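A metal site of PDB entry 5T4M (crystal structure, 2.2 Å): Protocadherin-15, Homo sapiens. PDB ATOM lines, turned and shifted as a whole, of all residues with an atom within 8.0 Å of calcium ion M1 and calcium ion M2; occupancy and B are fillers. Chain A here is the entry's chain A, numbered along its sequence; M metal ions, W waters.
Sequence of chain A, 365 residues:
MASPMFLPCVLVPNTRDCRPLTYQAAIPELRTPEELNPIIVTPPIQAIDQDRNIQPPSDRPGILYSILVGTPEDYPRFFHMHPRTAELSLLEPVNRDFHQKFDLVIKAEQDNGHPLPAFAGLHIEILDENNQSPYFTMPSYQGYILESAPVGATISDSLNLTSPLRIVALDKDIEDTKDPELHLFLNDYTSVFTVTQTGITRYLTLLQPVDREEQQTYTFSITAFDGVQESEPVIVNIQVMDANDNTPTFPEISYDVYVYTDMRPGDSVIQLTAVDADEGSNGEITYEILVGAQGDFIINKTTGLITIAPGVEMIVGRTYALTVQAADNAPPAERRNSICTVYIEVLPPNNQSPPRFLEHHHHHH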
ATOM      1  N   GLU A  29     -31.201 -34.339 -15.253  1.00  0.00           N
ATOM      2  CA  GLU A  29     -30.651 -34.332 -16.599  1.00  0.00           C
ATOM      3  C   GLU A  29     -29.190 -34.807 -16.614  1.00  0.00           C
ATOM      4  O   GLU A  29     -28.409 -34.447 -15.742  1.00  0.00           O
ATOM      5  CB  GLU A  29     -30.744 -32.921 -17.192  1.00  0.00           C
ATOM      6  CG  GLU A  29     -30.008 -32.734 -18.513  1.00  0.00           C
ATOM      7  CD  GLU A  29     -29.713 -31.279 -18.804  1.00  0.00           C
ATOM      8  OE1 GLU A  29     -29.519 -30.501 -17.854  1.00  0.00           O
ATOM      9  OE2 GLU A  29     -29.684 -30.913 -20.003  1.00  0.00           O
ATOM     10  N   ARG A  96     -32.109 -32.455 -21.383  1.00  0.00           N
ATOM     11  CA  ARG A  96     -33.327 -31.683 -21.219  1.00  0.00           C
ATOM     12  C   ARG A  96     -33.602 -30.765 -22.405  1.00  0.00           C
ATOM     13  O   ARG A  96     -34.745 -30.354 -22.619  1.00  0.00           O
ATOM     14  CB  ARG A  96     -33.277 -30.858 -19.931  1.00  0.00           C
ATOM     15  CG  ARG A  96     -34.648 -30.415 -19.461  1.00  0.00           C
ATOM     16  CD  ARG A  96     -34.602 -29.611 -18.177  1.00  0.00           C
ATOM     17  NE  ARG A  96     -35.949 -29.310 -17.709  1.00  0.00           N
ATOM     18  CZ  ARG A  96     -36.690 -28.309 -18.164  1.00  0.00           C
ATOM     19  NH1 ARG A  96     -36.213 -27.483 -19.081  1.00  0.00           N
ATOM     20  NH2 ARG A  96     -37.915 -28.116 -17.687  1.00  0.00           N
ATOM     21  N   LEU A 127     -35.212 -32.908 -14.907  1.00  0.00           N
ATOM     22  CA  LEU A 127     -34.828 -31.761 -14.087  1.00  0.00           C
ATOM     23  C   LEU A 127     -33.612 -31.004 -14.617  1.00  0.00           C
ATOM     24  O   LEU A 127     -32.623 -31.615 -15.023  1.00  0.00           O
ATOM     25  CB  LEU A 127     -34.542 -32.223 -12.653  1.00  0.00           C
ATOM     26  CG  LEU A 127     -35.668 -32.914 -11.892  1.00  0.00           C
ATOM     27  CD1 LEU A 127     -35.142 -33.491 -10.580  1.00  0.00           C
ATOM     28  CD2 LEU A 127     -36.827 -31.959 -11.633  1.00  0.00           C
ATOM     29  N   ASP A 128     -33.707 -29.682 -14.605  1.00  0.00           N
ATOM     30  CA  ASP A 128     -32.525 -28.832 -14.777  1.00  0.00           C
ATOM     31  C   ASP A 128     -31.603 -29.082 -13.592  1.00  0.00           C
ATOM     32  O   ASP A 128     -32.051 -29.376 -12.489  1.00  0.00           O
ATOM     33  CB  ASP A 128     -32.910 -27.347 -14.853  1.00  0.00           C
ATOM     34  CG  ASP A 128     -33.164 -26.875 -16.269  1.00  0.00           C
ATOM     35  OD1 ASP A 128     -32.302 -27.121 -17.139  1.00  0.00           O
ATOM     36  OD2 ASP A 128     -34.227 -26.268 -16.516  1.00  0.00           O
ATOM     37  N   GLU A 129     -30.303 -28.969 -13.821  1.00  0.00           N
ATOM     38  CA  GLU A 129     -29.335 -29.175 -12.752  1.00  0.00           C
ATOM     39  C   GLU A 129     -28.253 -28.100 -12.757  1.00  0.00           C
ATOM     40  O   GLU A 129     -27.973 -27.486 -13.783  1.00  0.00           O
ATOM     41  CB  GLU A 129     -28.686 -30.568 -12.875  1.00  0.00           C
ATOM     42  CG  GLU A 129     -29.644 -31.730 -12.668  1.00  0.00           C
ATOM     43  CD  GLU A 129     -30.209 -31.790 -11.257  1.00  0.00           C
ATOM     44  OE1 GLU A 129     -29.532 -31.314 -10.314  1.00  0.00           O
ATOM     45  OE2 GLU A 129     -31.331 -32.323 -11.078  1.00  0.00           O
ATOM     46  N   ASN A 130     -27.669 -27.880 -11.579  1.00  0.00           N
ATOM     47  CA  ASN A 130     -26.519 -26.995 -11.450  1.00  0.00           C
ATOM     48  C   ASN A 130     -25.303 -27.657 -12.068  1.00  0.00           C
ATOM     49  O   ASN A 130     -24.446 -28.181 -11.359  1.00  0.00           O
ATOM     50  CB  ASN A 130     -26.259 -26.668  -9.972  1.00  0.00           C
ATOM     51  CG  ASN A 130     -25.180 -25.605  -9.787  1.00  0.00           C
ATOM     52  OD1 ASN A 130     -24.380 -25.328 -10.686  1.00  0.00           O
ATOM     53  ND2 ASN A 130     -25.141 -25.026  -8.598  1.00  0.00           N
ATOM     54  N   ASN A 131     -25.231 -27.642 -13.399  1.00  0.00           N
ATOM     55  CA  ASN A 131     -24.209 -28.388 -14.121  1.00  0.00           C
ATOM     56  C   ASN A 131     -23.326 -27.509 -14.997  1.00  0.00           C
ATOM     57  O   ASN A 131     -22.642 -27.999 -15.894  1.00  0.00           O
ATOM     58  CB  ASN A 131     -24.860 -29.496 -14.963  1.00  0.00           C
ATOM     59  CG  ASN A 131     -26.123 -29.016 -15.674  1.00  0.00           C
ATOM     60  OD1 ASN A 131     -26.332 -27.823 -15.877  1.00  0.00           O
ATOM     61  ND2 ASN A 131     -26.975 -29.967 -16.053  1.00  0.00           N
ATOM     62  N   GLN A 132     -23.348 -26.209 -14.740  1.00  0.00           N
ATOM     63  CA  GLN A 132     -22.465 -25.273 -15.445  1.00  0.00           C
ATOM     64  C   GLN A 132     -21.564 -24.563 -14.440  1.00  0.00           C
ATOM     65  O   GLN A 132     -22.029 -24.016 -13.442  1.00  0.00           O
ATOM     66  CB  GLN A 132     -23.284 -24.251 -16.238  1.00  0.00           C
ATOM     67  CG  GLN A 132     -24.244 -24.849 -17.264  1.00  0.00           C
ATOM     68  CD  GLN A 132     -23.548 -25.382 -18.502  1.00  0.00           C
ATOM     69  OE1 GLN A 132     -22.720 -24.703 -19.107  1.00  0.00           O
ATOM     70  NE2 GLN A 132     -23.882 -26.608 -18.875  1.00  0.00           N
ATOM     71  N   SER A 133     -20.255 -24.578 -14.706  1.00  0.00           N
ATOM     72  CA  SER A 133     -19.298 -23.886 -13.841  1.00  0.00           C
ATOM     73  C   SER A 133     -19.451 -22.379 -13.974  1.00  0.00           C
ATOM     74  O   SER A 133     -19.623 -21.862 -15.080  1.00  0.00           O
ATOM     75  CB  SER A 133     -17.867 -24.297 -14.185  1.00  0.00           C
ATOM     76  OG  SER A 133     -17.646 -25.681 -13.940  1.00  0.00           O
ATOM     77  N   PRO A 134     -19.382 -21.664 -12.842  1.00  0.00           N
ATOM     78  CA  PRO A 134     -19.385 -20.202 -12.909  1.00  0.00           C
ATOM     79  C   PRO A 134     -18.115 -19.691 -13.599  1.00  0.00           C
ATOM     80  O   PRO A 134     -17.178 -20.459 -13.807  1.00  0.00           O
ATOM     81  CB  PRO A 134     -19.435 -19.792 -11.436  1.00  0.00           C
ATOM     82  CG  PRO A 134     -18.832 -20.943 -10.702  1.00  0.00           C
ATOM     83  CD  PRO A 134     -19.253 -22.161 -11.461  1.00  0.00           C
ATOM     84  N   TYR A 135     -18.105 -18.416 -13.957  1.00  0.00           N
ATOM     85  CA  TYR A 135     -16.976 -17.854 -14.683  1.00  0.00           C
ATOM     86  C   TYR A 135     -16.902 -16.344 -14.514  1.00  0.00           C
ATOM     87  O   TYR A 135     -17.903 -15.681 -14.236  1.00  0.00           O
ATOM     88  CB  TYR A 135     -17.059 -18.219 -16.170  1.00  0.00           C
ATOM     89  CG  TYR A 135     -18.242 -17.591 -16.900  1.00  0.00           C
ATOM     90  CD1 TYR A 135     -19.473 -18.238 -16.950  1.00  0.00           C
ATOM     91  CD2 TYR A 135     -18.112 -16.367 -17.544  1.00  0.00           C
ATOM     92  CE1 TYR A 135     -20.549 -17.667 -17.612  1.00  0.00           C
ATOM     93  CE2 TYR A 135     -19.186 -15.786 -18.208  1.00  0.00           C
ATOM     94  CZ  TYR A 135     -20.390 -16.442 -18.235  1.00  0.00           C
ATOM     95  OH  TYR A 135     -21.456 -15.873 -18.896  1.00  0.00           O
ATOM     96  N   LEU A 170     -20.476 -14.701 -13.445  1.00  0.00           N
ATOM     97  CA  LEU A 170     -21.738 -15.220 -13.945  1.00  0.00           C
ATOM     98  C   LEU A 170     -21.786 -16.744 -13.913  1.00  0.00           C
ATOM     99  O   LEU A 170     -20.787 -17.390 -13.584  1.00  0.00           O
ATOM    100  CB  LEU A 170     -21.977 -14.725 -15.378  1.00  0.00           C
ATOM    101  CG  LEU A 170     -22.212 -13.230 -15.539  1.00  0.00           C
ATOM    102  CD1 LEU A 170     -22.476 -12.874 -16.996  1.00  0.00           C
ATOM    103  CD2 LEU A 170     -23.361 -12.777 -14.666  1.00  0.00           C
ATOM    104  N   ASP A 171     -22.944 -17.303 -14.246  1.00  0.00           N
ATOM    105  CA  ASP A 171     -23.160 -18.753 -14.224  1.00  0.00           C
ATOM    106  C   ASP A 171     -24.332 -19.089 -15.147  1.00  0.00           C
ATOM    107  O   ASP A 171     -25.437 -18.571 -14.975  1.00  0.00           O
ATOM    108  CB  ASP A 171     -23.450 -19.234 -12.789  1.00  0.00           C
ATOM    109  CG  ASP A 171     -23.361 -20.752 -12.633  1.00  0.00           C
ATOM    110  OD1 ASP A 171     -23.903 -21.501 -13.469  1.00  0.00           O
ATOM    111  OD2 ASP A 171     -22.741 -21.201 -11.635  1.00  0.00           O
ATOM    112  N   LYS A 172     -24.080 -19.948 -16.134  1.00  0.00           N
ATOM    113  CA  LYS A 172     -25.077 -20.252 -17.157  1.00  0.00           C
ATOM    114  C   LYS A 172     -26.310 -20.995 -16.632  1.00  0.00           C
ATOM    115  O   LYS A 172     -27.307 -21.097 -17.337  1.00  0.00           O
ATOM    116  CB  LYS A 172     -24.449 -21.062 -18.300  1.00  0.00           C
ATOM    117  CG  LYS A 172     -23.593 -20.240 -19.254  1.00  0.00           C
ATOM    118  CD  LYS A 172     -24.417 -19.152 -19.920  1.00  0.00           C
ATOM    119  CE  LYS A 172     -23.562 -18.260 -20.810  1.00  0.00           C
ATOM    120  NZ  LYS A 172     -22.917 -19.021 -21.914  1.00  0.00           N
ATOM    121  N   ASP A 173     -26.237 -21.514 -15.411  1.00  0.00           N
ATOM    122  CA  ASP A 173     -27.387 -22.168 -14.806  1.00  0.00           C
ATOM    123  C   ASP A 173     -28.401 -21.129 -14.320  1.00  0.00           C
ATOM    124  O   ASP A 173     -29.565 -21.444 -14.108  1.00  0.00           O
ATOM    125  CB  ASP A 173     -26.956 -23.070 -13.634  1.00  0.00           C
ATOM    126  CG  ASP A 173     -26.191 -24.286 -14.105  1.00  0.00           C
ATOM    127  OD1 ASP A 173     -26.551 -24.846 -15.157  1.00  0.00           O
ATOM    128  OD2 ASP A 173     -25.230 -24.699 -13.415  1.00  0.00           O
ATOM    129  N   ILE A 174     -27.922 -19.904 -14.153  1.00  0.00           N
ATOM    130  CA  ILE A 174     -28.759 -18.800 -13.683  1.00  0.00           C
ATOM    131  C   ILE A 174     -29.124 -17.867 -14.843  1.00  0.00           C
ATOM    132  O   ILE A 174     -28.259 -17.477 -15.627  1.00  0.00           O
ATOM    133  CB  ILE A 174     -28.037 -17.986 -12.584  1.00  0.00           C
ATOM    134  CG1 ILE A 174     -27.505 -18.918 -11.486  1.00  0.00           C
ATOM    135  CG2 ILE A 174     -28.961 -16.927 -11.998  1.00  0.00           C
ATOM    136  CD1 ILE A 174     -28.563 -19.761 -10.807  1.00  0.00           C
ATOM    137  N   PRO A 180     -26.470 -14.811  -9.386  1.00  0.00           N
ATOM    138  CA  PRO A 180     -26.136 -16.244  -9.313  1.00  0.00           C
ATOM    139  C   PRO A 180     -25.788 -16.701  -7.890  1.00  0.00           C
ATOM    140  O   PRO A 180     -25.600 -17.894  -7.666  1.00  0.00           O
ATOM    141  CB  PRO A 180     -24.921 -16.368 -10.245  1.00  0.00           C
ATOM    142  CG  PRO A 180     -24.298 -15.020 -10.214  1.00  0.00           C
ATOM    143  CD  PRO A 180     -25.435 -14.044 -10.095  1.00  0.00           C
ATOM    144  N   LEU A 182     -23.093 -16.519  -5.981  1.00  0.00           N
ATOM    145  CA  LEU A 182     -21.854 -17.284  -5.950  1.00  0.00           C
ATOM    146  C   LEU A 182     -21.059 -16.999  -4.684  1.00  0.00           C
ATOM    147  O   LEU A 182     -21.175 -15.928  -4.096  1.00  0.00           O
ATOM    148  CB  LEU A 182     -21.004 -16.960  -7.182  1.00  0.00           C
ATOM    149  CG  LEU A 182     -21.683 -17.248  -8.529  1.00  0.00           C
ATOM    150  CD1 LEU A 182     -20.845 -16.686  -9.671  1.00  0.00           C
ATOM    151  CD2 LEU A 182     -21.908 -18.746  -8.692  1.00  0.00           C
ATOM    152  N   PHE A 225     -17.635 -20.118  -6.751  1.00  0.00           N
ATOM    153  CA  PHE A 225     -18.182 -21.425  -6.378  1.00  0.00           C
ATOM    154  C   PHE A 225     -19.716 -21.374  -6.309  1.00  0.00           C
ATOM    155  O   PHE A 225     -20.276 -20.474  -5.678  1.00  0.00           O
ATOM    156  CB  PHE A 225     -17.594 -21.882  -5.046  1.00  0.00           C
ATOM    157  CG  PHE A 225     -18.100 -23.213  -4.572  1.00  0.00           C
ATOM    158  CD1 PHE A 225     -17.906 -24.359  -5.336  1.00  0.00           C
ATOM    159  CD2 PHE A 225     -18.756 -23.328  -3.354  1.00  0.00           C
ATOM    160  CE1 PHE A 225     -18.360 -25.581  -4.892  1.00  0.00           C
ATOM    161  CE2 PHE A 225     -19.211 -24.562  -2.916  1.00  0.00           C
ATOM    162  CZ  PHE A 225     -19.013 -25.689  -3.685  1.00  0.00           C
ATOM    163  N   ASP A 226     -20.369 -22.327  -6.967  1.00  0.00           N
ATOM    164  CA  ASP A 226     -21.837 -22.304  -7.067  1.00  0.00           C
ATOM    165  C   ASP A 226     -22.517 -23.355  -6.204  1.00  0.00           C
ATOM    166  O   ASP A 226     -23.720 -23.614  -6.360  1.00  0.00           O
ATOM    167  CB  ASP A 226     -22.274 -22.485  -8.534  1.00  0.00           C
ATOM    168  CG  ASP A 226     -21.829 -23.817  -9.131  1.00  0.00           C
ATOM    169  OD1 ASP A 226     -21.305 -24.689  -8.402  1.00  0.00           O
ATOM    170  OD2 ASP A 226     -22.005 -23.997 -10.358  1.00  0.00           O
ATOM    171  N   GLY A 227     -21.761 -23.975  -5.304  1.00  0.00           N
ATOM    172  CA  GLY A 227     -22.298 -25.030  -4.460  1.00  0.00           C
ATOM    173  C   GLY A 227     -21.989 -26.411  -4.993  1.00  0.00           C
ATOM    174  O   GLY A 227     -22.139 -27.401  -4.278  1.00  0.00           O
ATOM    175  N   VAL A 228     -21.553 -26.492  -6.242  1.00  0.00           N
ATOM    176  CA  VAL A 228     -21.230 -27.774  -6.864  1.00  0.00           C
ATOM    177  C   VAL A 228     -19.862 -27.765  -7.541  1.00  0.00           C
ATOM    178  O   VAL A 228     -19.044 -28.647  -7.325  1.00  0.00           O
ATOM    179  CB  VAL A 228     -22.299 -28.193  -7.898  1.00  0.00           C
ATOM    180  CG1 VAL A 228     -21.960 -29.546  -8.501  1.00  0.00           C
ATOM    181  CG2 VAL A 228     -23.678 -28.222  -7.268  1.00  0.00           C
ATOM    182  N   GLN A 229     -19.639 -26.751  -8.386  1.00  0.00           N
ATOM    183  CA  GLN A 229     -18.402 -26.657  -9.159  1.00  0.00           C
ATOM    184  C   GLN A 229     -17.685 -25.334  -8.914  1.00  0.00           C
ATOM    185  O   GLN A 229     -18.313 -24.315  -8.637  1.00  0.00           O
ATOM    186  CB  GLN A 229     -18.682 -26.824 -10.650  1.00  0.00           C
ATOM    187  CG  GLN A 229     -19.310 -28.152 -11.038  1.00  0.00           C
ATOM    188  CD  GLN A 229     -20.772 -28.034 -11.444  1.00  0.00           C
ATOM    189  OE1 GLN A 229     -21.363 -26.950 -11.403  1.00  0.00           O
ATOM    190  NE2 GLN A 229     -21.359 -29.150 -11.839  1.00  0.00           N
HETATM  191 CA    CA M   1     -23.748 -23.418 -11.929  1.00  0.00          CA
HETATM  192 CA    CA M   2     -28.192 -26.358 -15.907  1.00  0.00          CA
HETATM  193  O   HOH W   1     -27.598 -26.002 -18.229  1.00  0.00           O
HETATM  194  O   HOH W   2     -29.746 -28.019 -16.709  1.00  0.00           O
HETATM  195  O   HOH W   3     -25.509 -22.419 -10.680  1.00  0.00           O
HETATM  196  O   HOH W   4     -29.363 -24.506 -17.023  1.00  0.00           O
HETATM  197  O   HOH W   5     -29.970 -25.442 -14.626  1.00  0.00           O
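N of Val 228 sits at hydrogen-bond distance from OD1 of Asp 226.
OD1 of Asp 226 lies within hydrogen-bond range of N of Gln 229, 2.7 Å away.
ND2 of Asn 131 is in hydrogen-bond range of OE1 of Glu 29.
NE2 of Gln 229 lies within hydrogen-bond range of O of Asn 130, at 3.3 Å.
Of the 23 residues printed, 5 come within 4 Å of calcium ion M1.
Of the 23 residues printed, 3 come within 4 Å of calcium ion M2.
The nearest printed residue that does not touch calcium ion M2 is Asp 128 (4.4 Å).
Calcium ion M1 is bound by OD1 of Asn 130 (2.4 Å), O of Gln 132 (2.4 Å), water W3 (2.4 Å), OD2 of Asp 226 (2.4 Å), OD2 of Asp 171 (2.5 Å), OD2 of Asp 173 (2.5 Å) and OD1 of Asp 171 (2.5 Å).
Calcium ion M2 is bound by OD1 of Asp 173 (2.4 Å), OD1 of Asn 131 (2.4 Å), water W5 (2.4 Å), water W2 (2.4 Å), O of Glu 129 (2.4 Å), water W1 (2.4 Å) and water W4 (2.5 Å).
Water W2 lies within hydrogen-bond range of OE1 of Glu 29 (2.7 Å), OD1 of Asp 128 (2.7 Å), N of Glu 129 (3.1 Å) and ND2 of Asn 131 (3.5 Å).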
